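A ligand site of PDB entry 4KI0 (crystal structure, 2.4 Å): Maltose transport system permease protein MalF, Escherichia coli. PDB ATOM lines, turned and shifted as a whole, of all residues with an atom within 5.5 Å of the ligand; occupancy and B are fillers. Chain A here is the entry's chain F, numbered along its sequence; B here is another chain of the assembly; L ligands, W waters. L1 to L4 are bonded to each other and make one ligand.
Water W6 bridges the side-chain amide nitrogen of Asn 440 (2.7 Å) and an oxygen (O3) of LG4 L4 (2.8 Å). Water W3 lies within hydrogen-bond range of the backbone carbonyl oxygen of Gly 380 and an oxygen (O5) of LG4 L4. Water W9 bridges the side-chain hydroxyl (OH) of Tyr 325 (2.5 Å) and an oxygen (O1) of LG3 L3 (3.0 Å). Water W1 lies within hydrogen-bond range of OH of Tyr 383 (2.7 Å), O5 of LG2 L2 (3.0 Å) and O of Leu 429 (3.0 Å). Water W4 lies within hydrogen-bond range of the backbone carbonyl oxygen of Ala 432 (3.3 Å) and an oxygen (O4) of LG2 L2 (3.5 Å).
OD1 of Asn 376 is in hydrogen-bond range of ND2 of Asn 437. OD1 of Asn 376 lies within hydrogen-bond range of OG1 of Thr 291 (3.1 Å). The side-chain amide oxygen of Asn 437 sits close to the backbone carbonyl oxygen of Ser 433 (3.2 Å). OD1 of Asn 440 is in hydrogen-bond range of ND2 of Asn 437, at 3.0 Å. O of Thr 291 lies within hydrogen-bond range of OG1 of Thr 295, at 2.7 Å.
O2 of LG3 L3 is in hydrogen-bond range of OH of Tyr 325 (2.5 Å). ND2 of Asn 376 is in hydrogen-bond range of O3 of LG4 L4 (2.6 Å). The side-chain hydroxyl of Ser 433 is in hydrogen-bond range of an oxygen (O5) of LG3 L3, 2.8 Å away. OD1 of Asn 440 sits at hydrogen-bond distance from O3 of LG4 L4, 2.8 Å away. The side-chain amide oxygen of Asn 437 lies within hydrogen-bond range of an oxygen (O5) of LG4 L4.
Residues that only touch the ligand: Gly 380, Ala 432, Tyr 383, Thr 291, Phe 436, Gln 129 of chain B, Leu 379 and Leu 172 of chain B. Hydrophobic or aromatic side chains that line the ligand: Tyr 325, Leu 379, Tyr 383, Ala 432, Phe 436 and Leu 172 of chain B. The nearest printed residue that does not touch the ligand is Thr 295 (4.4 Å).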
ATOM      1  N   THR A 291      -0.071   1.620  13.492  1.00  0.00           N
ATOM      2  CA  THR A 291      -1.337   2.282  13.831  1.00  0.00           C
ATOM      3  C   THR A 291      -1.449   2.429  15.348  1.00  0.00           C
ATOM      4  O   THR A 291      -1.729   3.519  15.864  1.00  0.00           O
ATOM      5  CB  THR A 291      -2.559   1.491  13.304  1.00  0.00           C
ATOM      6  OG1 THR A 291      -2.568   1.502  11.873  1.00  0.00           O
ATOM      7  CG2 THR A 291      -3.858   2.086  13.827  1.00  0.00           C
ATOM      8  N   THR A 295      -1.361   6.074  17.206  1.00  0.00           N
ATOM      9  CA  THR A 295      -2.611   6.501  17.869  1.00  0.00           C
ATOM     10  C   THR A 295      -2.416   6.672  19.372  1.00  0.00           C
ATOM     11  O   THR A 295      -2.920   7.631  19.963  1.00  0.00           O
ATOM     12  CB  THR A 295      -3.800   5.547  17.595  1.00  0.00           C
ATOM     13  OG1 THR A 295      -3.415   4.181  17.855  1.00  0.00           O
ATOM     14  CG2 THR A 295      -4.248   5.674  16.153  1.00  0.00           C
ATOM     15  N   TYR A 325     -13.697  11.676  15.323  1.00  0.00           N
ATOM     16  CA  TYR A 325     -14.363  10.497  15.845  1.00  0.00           C
ATOM     17  C   TYR A 325     -15.865  10.722  15.977  1.00  0.00           C
ATOM     18  O   TYR A 325     -16.629   9.768  16.079  1.00  0.00           O
ATOM     19  CB  TYR A 325     -13.731  10.159  17.189  1.00  0.00           C
ATOM     20  CG  TYR A 325     -13.900   8.751  17.715  1.00  0.00           C
ATOM     21  CD1 TYR A 325     -14.165   7.657  16.879  1.00  0.00           C
ATOM     22  CD2 TYR A 325     -13.758   8.499  19.075  1.00  0.00           C
ATOM     23  CE1 TYR A 325     -14.296   6.382  17.391  1.00  0.00           C
ATOM     24  CE2 TYR A 325     -13.884   7.235  19.595  1.00  0.00           C
ATOM     25  CZ  TYR A 325     -14.149   6.184  18.752  1.00  0.00           C
ATOM     26  OH  TYR A 325     -14.273   4.926  19.301  1.00  0.00           O
ATOM     27  N   SER A 329     -16.999   7.376  10.033  1.00  0.00           N
ATOM     28  CA  SER A 329     -15.746   7.265   9.314  1.00  0.00           C
ATOM     29  C   SER A 329     -15.946   7.035   7.818  1.00  0.00           C
ATOM     30  O   SER A 329     -15.060   7.349   7.014  1.00  0.00           O
ATOM     31  CB  SER A 329     -14.905   6.118   9.899  1.00  0.00           C
ATOM     32  OG  SER A 329     -15.484   4.850   9.621  1.00  0.00           O
ATOM     33  N   ASN A 376      -5.525   6.244   9.060  1.00  0.00           N
ATOM     34  CA  ASN A 376      -5.896   5.434  10.220  1.00  0.00           C
ATOM     35  C   ASN A 376      -5.550   6.140  11.530  1.00  0.00           C
ATOM     36  O   ASN A 376      -6.288   6.041  12.516  1.00  0.00           O
ATOM     37  CB  ASN A 376      -5.217   4.060  10.148  1.00  0.00           C
ATOM     38  CG  ASN A 376      -6.075   2.960  10.747  1.00  0.00           C
ATOM     39  OD1 ASN A 376      -5.571   1.885  11.081  1.00  0.00           O
ATOM     40  ND2 ASN A 376      -7.359   3.210  10.877  1.00  0.00           N
ATOM     41  N   LEU A 379      -8.138   8.616  12.060  1.00  0.00           N
ATOM     42  CA  LEU A 379      -9.305   7.877  12.554  1.00  0.00           C
ATOM     43  C   LEU A 379      -9.184   7.440  14.015  1.00  0.00           C
ATOM     44  O   LEU A 379     -10.161   7.501  14.765  1.00  0.00           O
ATOM     45  CB  LEU A 379      -9.545   6.632  11.671  1.00  0.00           C
ATOM     46  CG  LEU A 379     -10.031   6.840  10.237  1.00  0.00           C
ATOM     47  CD1 LEU A 379      -9.934   5.560   9.422  1.00  0.00           C
ATOM     48  CD2 LEU A 379     -11.457   7.371  10.246  1.00  0.00           C
ATOM     49  N   GLY A 380      -7.986   7.018  14.424  1.00  0.00           N
ATOM     50  CA  GLY A 380      -7.798   6.273  15.678  1.00  0.00           C
ATOM     51  C   GLY A 380      -7.295   7.028  16.891  1.00  0.00           C
ATOM     52  O   GLY A 380      -7.465   6.569  18.023  1.00  0.00           O
ATOM     53  N   TYR A 383      -9.797   7.957  20.004  1.00  0.00           N
ATOM     54  CA  TYR A 383     -10.073   6.833  20.892  1.00  0.00           C
ATOM     55  C   TYR A 383      -9.037   6.764  21.993  1.00  0.00           C
ATOM     56  O   TYR A 383      -9.364   6.683  23.171  1.00  0.00           O
ATOM     57  CB  TYR A 383     -10.039   5.540  20.091  1.00  0.00           C
ATOM     58  CG  TYR A 383     -10.201   4.286  20.887  1.00  0.00           C
ATOM     59  CD1 TYR A 383     -11.375   4.017  21.583  1.00  0.00           C
ATOM     60  CD2 TYR A 383      -9.192   3.330  20.924  1.00  0.00           C
ATOM     61  CE1 TYR A 383     -11.536   2.858  22.300  1.00  0.00           C
ATOM     62  CE2 TYR A 383      -9.350   2.152  21.652  1.00  0.00           C
ATOM     63  CZ  TYR A 383     -10.531   1.922  22.326  1.00  0.00           C
ATOM     64  OH  TYR A 383     -10.695   0.771  23.049  1.00  0.00           O
ATOM     65  N   MET A 384      -7.765   6.810  21.583  1.00  0.00           N
ATOM     66  CA  MET A 384      -6.671   6.671  22.525  1.00  0.00           C
ATOM     67  C   MET A 384      -6.554   7.888  23.422  1.00  0.00           C
ATOM     68  O   MET A 384      -6.225   7.765  24.595  1.00  0.00           O
ATOM     69  CB  MET A 384      -5.368   6.382  21.777  1.00  0.00           C
ATOM     70  CG  MET A 384      -5.265   4.934  21.334  1.00  0.00           C
ATOM     71  SD  MET A 384      -5.353   3.834  22.759  1.00  0.00           S
ATOM     72  CE  MET A 384      -5.592   2.224  22.021  1.00  0.00           C
ATOM     73  N   LEU A 429      -5.780  -2.583  26.178  1.00  0.00           N
ATOM     74  CA  LEU A 429      -6.414  -1.767  25.139  1.00  0.00           C
ATOM     75  C   LEU A 429      -5.600  -1.719  23.849  1.00  0.00           C
ATOM     76  O   LEU A 429      -6.180  -1.686  22.767  1.00  0.00           O
ATOM     77  CB  LEU A 429      -6.633  -0.342  25.650  1.00  0.00           C
ATOM     78  CG  LEU A 429      -7.572  -0.225  26.847  1.00  0.00           C
ATOM     79  CD1 LEU A 429      -7.377   1.134  27.503  1.00  0.00           C
ATOM     80  CD2 LEU A 429      -9.023  -0.435  26.460  1.00  0.00           C
ATOM     81  N   ALA A 432      -5.931  -5.129  22.129  1.00  0.00           N
ATOM     82  CA  ALA A 432      -7.229  -5.141  21.469  1.00  0.00           C
ATOM     83  C   ALA A 432      -7.175  -4.343  20.171  1.00  0.00           C
ATOM     84  O   ALA A 432      -7.671  -4.789  19.118  1.00  0.00           O
ATOM     85  CB  ALA A 432      -8.292  -4.575  22.394  1.00  0.00           C
ATOM     86  N   SER A 433      -6.589  -3.152  20.247  1.00  0.00           N
ATOM     87  CA  SER A 433      -6.476  -2.293  19.069  1.00  0.00           C
ATOM     88  C   SER A 433      -5.665  -2.981  17.965  1.00  0.00           C
ATOM     89  O   SER A 433      -5.963  -2.814  16.787  1.00  0.00           O
ATOM     90  CB  SER A 433      -5.877  -0.944  19.430  1.00  0.00           C
ATOM     91  OG  SER A 433      -6.003  -0.012  18.361  1.00  0.00           O
ATOM     92  N   PHE A 434      -4.658  -3.771  18.341  1.00  0.00           N
ATOM     93  CA  PHE A 434      -3.854  -4.514  17.383  1.00  0.00           C
ATOM     94  C   PHE A 434      -4.703  -5.558  16.645  1.00  0.00           C
ATOM     95  O   PHE A 434      -4.629  -5.669  15.423  1.00  0.00           O
ATOM     96  CB  PHE A 434      -2.668  -5.211  18.062  1.00  0.00           C
ATOM     97  CG  PHE A 434      -1.884  -6.093  17.139  1.00  0.00           C
ATOM     98  CD1 PHE A 434      -2.185  -7.438  17.007  1.00  0.00           C
ATOM     99  CD2 PHE A 434      -0.856  -5.565  16.368  1.00  0.00           C
ATOM    100  CE1 PHE A 434      -1.478  -8.247  16.135  1.00  0.00           C
ATOM    101  CE2 PHE A 434      -0.130  -6.368  15.500  1.00  0.00           C
ATOM    102  CZ  PHE A 434      -0.435  -7.712  15.382  1.00  0.00           C
ATOM    103  N   PHE A 436      -8.104  -5.579  16.331  1.00  0.00           N
ATOM    104  CA  PHE A 436      -9.054  -4.832  15.495  1.00  0.00           C
ATOM    105  C   PHE A 436      -8.368  -4.399  14.207  1.00  0.00           C
ATOM    106  O   PHE A 436      -8.834  -4.703  13.120  1.00  0.00           O
ATOM    107  CB  PHE A 436      -9.600  -3.606  16.238  1.00  0.00           C
ATOM    108  CG  PHE A 436     -10.544  -2.744  15.411  1.00  0.00           C
ATOM    109  CD1 PHE A 436     -10.062  -1.691  14.648  1.00  0.00           C
ATOM    110  CD2 PHE A 436     -11.916  -2.970  15.432  1.00  0.00           C
ATOM    111  CE1 PHE A 436     -10.919  -0.894  13.898  1.00  0.00           C
ATOM    112  CE2 PHE A 436     -12.786  -2.174  14.694  1.00  0.00           C
ATOM    113  CZ  PHE A 436     -12.288  -1.134  13.923  1.00  0.00           C
ATOM    114  N   ASN A 437      -7.241  -3.717  14.322  1.00  0.00           N
ATOM    115  CA  ASN A 437      -6.564  -3.192  13.137  1.00  0.00           C
ATOM    116  C   ASN A 437      -6.004  -4.274  12.238  1.00  0.00           C
ATOM    117  O   ASN A 437      -5.897  -4.083  11.037  1.00  0.00           O
ATOM    118  CB  ASN A 437      -5.495  -2.167  13.509  1.00  0.00           C
ATOM    119  CG  ASN A 437      -6.085  -0.789  13.746  1.00  0.00           C
ATOM    120  OD1 ASN A 437      -5.959  -0.220  14.844  1.00  0.00           O
ATOM    121  ND2 ASN A 437      -6.744  -0.252  12.716  1.00  0.00           N
ATOM    122  N   ASN A 440      -8.854  -4.756   9.860  1.00  0.00           N
ATOM    123  CA  ASN A 440      -9.536  -3.506   9.512  1.00  0.00           C
ATOM    124  C   ASN A 440      -9.929  -3.493   8.026  1.00  0.00           C
ATOM    125  O   ASN A 440      -9.466  -2.654   7.257  1.00  0.00           O
ATOM    126  CB  ASN A 440      -8.663  -2.311   9.866  1.00  0.00           C
ATOM    127  CG  ASN A 440      -9.466  -1.047  10.104  1.00  0.00           C
ATOM    128  OD1 ASN A 440      -9.047  -0.159  10.870  1.00  0.00           O
ATOM    129  ND2 ASN A 440     -10.622  -0.943   9.468  1.00  0.00           N
ATOM    130  N   LEU A 443     -11.343  -0.072   5.994  1.00  0.00           N
ATOM    131  CA  LEU A 443     -10.454   1.038   5.662  1.00  0.00           C
ATOM    132  C   LEU A 443      -9.776   0.795   4.321  1.00  0.00           C
ATOM    133  O   LEU A 443      -9.777   1.670   3.471  1.00  0.00           O
ATOM    134  CB  LEU A 443      -9.406   1.271   6.733  1.00  0.00           C
ATOM    135  CG  LEU A 443      -8.319   2.302   6.385  1.00  0.00           C
ATOM    136  CD1 LEU A 443      -8.913   3.654   5.988  1.00  0.00           C
ATOM    137  CD2 LEU A 443      -7.348   2.479   7.538  1.00  0.00           C
ATOM    138  N   GLN B 129     -13.683 -11.533  22.394  1.00  0.00           N
ATOM    139  CA  GLN B 129     -14.136 -10.316  21.706  1.00  0.00           C
ATOM    140  C   GLN B 129     -13.263  -9.992  20.491  1.00  0.00           C
ATOM    141  O   GLN B 129     -13.642  -9.182  19.650  1.00  0.00           O
ATOM    142  CB  GLN B 129     -14.189  -9.121  22.671  1.00  0.00           C
ATOM    143  CG  GLN B 129     -15.156  -8.036  22.199  1.00  0.00           C
ATOM    144  CD  GLN B 129     -15.005  -6.719  22.959  1.00  0.00           C
ATOM    145  OE1 GLN B 129     -13.975  -6.470  23.587  1.00  0.00           O
ATOM    146  NE2 GLN B 129     -16.035  -5.880  22.888  1.00  0.00           N
ATOM    147  N   LEU B 172     -13.870  -4.916  26.877  1.00  0.00           N
ATOM    148  CA  LEU B 172     -12.782  -3.932  26.949  1.00  0.00           C
ATOM    149  C   LEU B 172     -13.057  -2.934  28.064  1.00  0.00           C
ATOM    150  O   LEU B 172     -12.155  -2.567  28.810  1.00  0.00           O
ATOM    151  CB  LEU B 172     -12.550  -3.226  25.602  1.00  0.00           C
ATOM    152  CG  LEU B 172     -11.287  -3.650  24.831  1.00  0.00           C
ATOM    153  CD1 LEU B 172     -10.035  -3.547  25.703  1.00  0.00           C
ATOM    154  CD2 LEU B 172     -11.437  -5.058  24.276  1.00  0.00           C
ATOM    155  N   ALA B 225     -19.775   4.837  19.859  1.00  0.00           N
ATOM    156  CA  ALA B 225     -19.998   3.557  19.222  1.00  0.00           C
ATOM    157  C   ALA B 225     -21.457   3.414  18.735  1.00  0.00           C
ATOM    158  O   ALA B 225     -21.690   3.157  17.551  1.00  0.00           O
ATOM    159  CB  ALA B 225     -19.624   2.433  20.171  1.00  0.00           C
HETATM  160  O1  LIG L   1     -14.401  -5.899  18.061  1.00  0.00           O
HETATM  161  C1  LG2 L   2     -14.145  -4.805  18.983  1.00  0.00           C
HETATM  162  C2  LG2 L   2     -15.275  -3.870  19.397  1.00  0.00           C
HETATM  163  C3  LG2 L   2     -14.896  -2.398  19.215  1.00  0.00           C
HETATM  164  C4  LG2 L   2     -13.429  -2.073  19.525  1.00  0.00           C
HETATM  165  C5  LG2 L   2     -12.418  -3.174  19.101  1.00  0.00           C
HETATM  166  C6  LG2 L   2     -11.002  -2.988  19.629  1.00  0.00           C
HETATM  167  O1  LG2 L   2     -16.419  -4.174  18.641  1.00  0.00           O
HETATM  168  O2  LG2 L   2     -15.703  -1.578  20.044  1.00  0.00           O
HETATM  169  O3  LG2 L   2     -13.163  -0.891  18.789  1.00  0.00           O
HETATM  170  O4  LG2 L   2     -12.842  -4.477  19.439  1.00  0.00           O
HETATM  171  O5  LG2 L   2     -10.989  -2.885  21.032  1.00  0.00           O
HETATM  172  C1  LG3 L   3     -12.585   0.172  19.560  1.00  0.00           C
HETATM  173  C2  LG3 L   3     -13.318   1.474  19.273  1.00  0.00           C
HETATM  174  C3  LG3 L   3     -13.097   1.899  17.834  1.00  0.00           C
HETATM  175  C4  LG3 L   3     -11.603   1.961  17.550  1.00  0.00           C
HETATM  176  C5  LG3 L   3     -10.902   0.661  17.925  1.00  0.00           C
HETATM  177  C6  LG3 L   3      -9.393   0.858  17.812  1.00  0.00           C
HETATM  178  O1  LG3 L   3     -14.706   1.323  19.494  1.00  0.00           O
HETATM  179  O2  LG3 L   3     -13.720   3.150  17.598  1.00  0.00           O
HETATM  180  O3  LG3 L   3     -11.373   2.156  16.182  1.00  0.00           O
HETATM  181  O4  LG3 L   3     -11.212   0.302  19.249  1.00  0.00           O
HETATM  182  O5  LG3 L   3      -8.765  -0.280  18.338  1.00  0.00           O
HETATM  183  C1  LG4 L   4     -10.983   3.496  15.807  1.00  0.00           C
HETATM  184  C2  LG4 L   4     -11.822   3.914  14.603  1.00  0.00           C
HETATM  185  C3  LG4 L   4     -11.433   3.092  13.370  1.00  0.00           C
HETATM  186  C4  LG4 L   4      -9.918   3.149  13.182  1.00  0.00           C
HETATM  187  C5  LG4 L   4      -9.216   2.715  14.447  1.00  0.00           C
HETATM  188  C6  LG4 L   4      -7.694   2.760  14.335  1.00  0.00           C
HETATM  189  O1  LG4 L   4     -13.184   3.750  14.914  1.00  0.00           O
HETATM  190  O2  LG4 L   4     -12.078   3.595  12.230  1.00  0.00           O
HETATM  191  O3  LG4 L   4      -9.534   2.352  12.078  1.00  0.00           O
HETATM  192  O4  LG4 L   4      -9.609   3.594  15.485  1.00  0.00           O
HETATM  193  O5  LG4 L   4      -7.111   2.331  15.552  1.00  0.00           O
HETATM  194  O   HOH W   1      -8.924  -0.897  21.853  1.00  0.00           O
HETATM  195  O   HOH W   2     -13.869   1.808  10.992  1.00  0.00           O
HETATM  196  O   HOH W   3      -7.183   3.870  17.930  1.00  0.00           O
HETATM  197  O   HOH W   4     -10.267  -6.817  19.561  1.00  0.00           O
HETATM  198  O   HOH W   5     -15.121   1.565  14.532  1.00  0.00           O
HETATM  199  O   HOH W   6     -11.278   1.637   9.984  1.00  0.00           O
HETATM  200  O   HOH W   7     -13.911   5.879  13.534  1.00  0.00           O
HETATM  201  O   HOH W   8     -18.733  -5.490  16.833  1.00  0.00           O
HETATM  202  O   HOH W   9     -15.774   3.707  20.921  1.00  0.00           O
HETATM  203  O   HOH W  10     -17.039   2.491  17.851  1.00  0.00           O
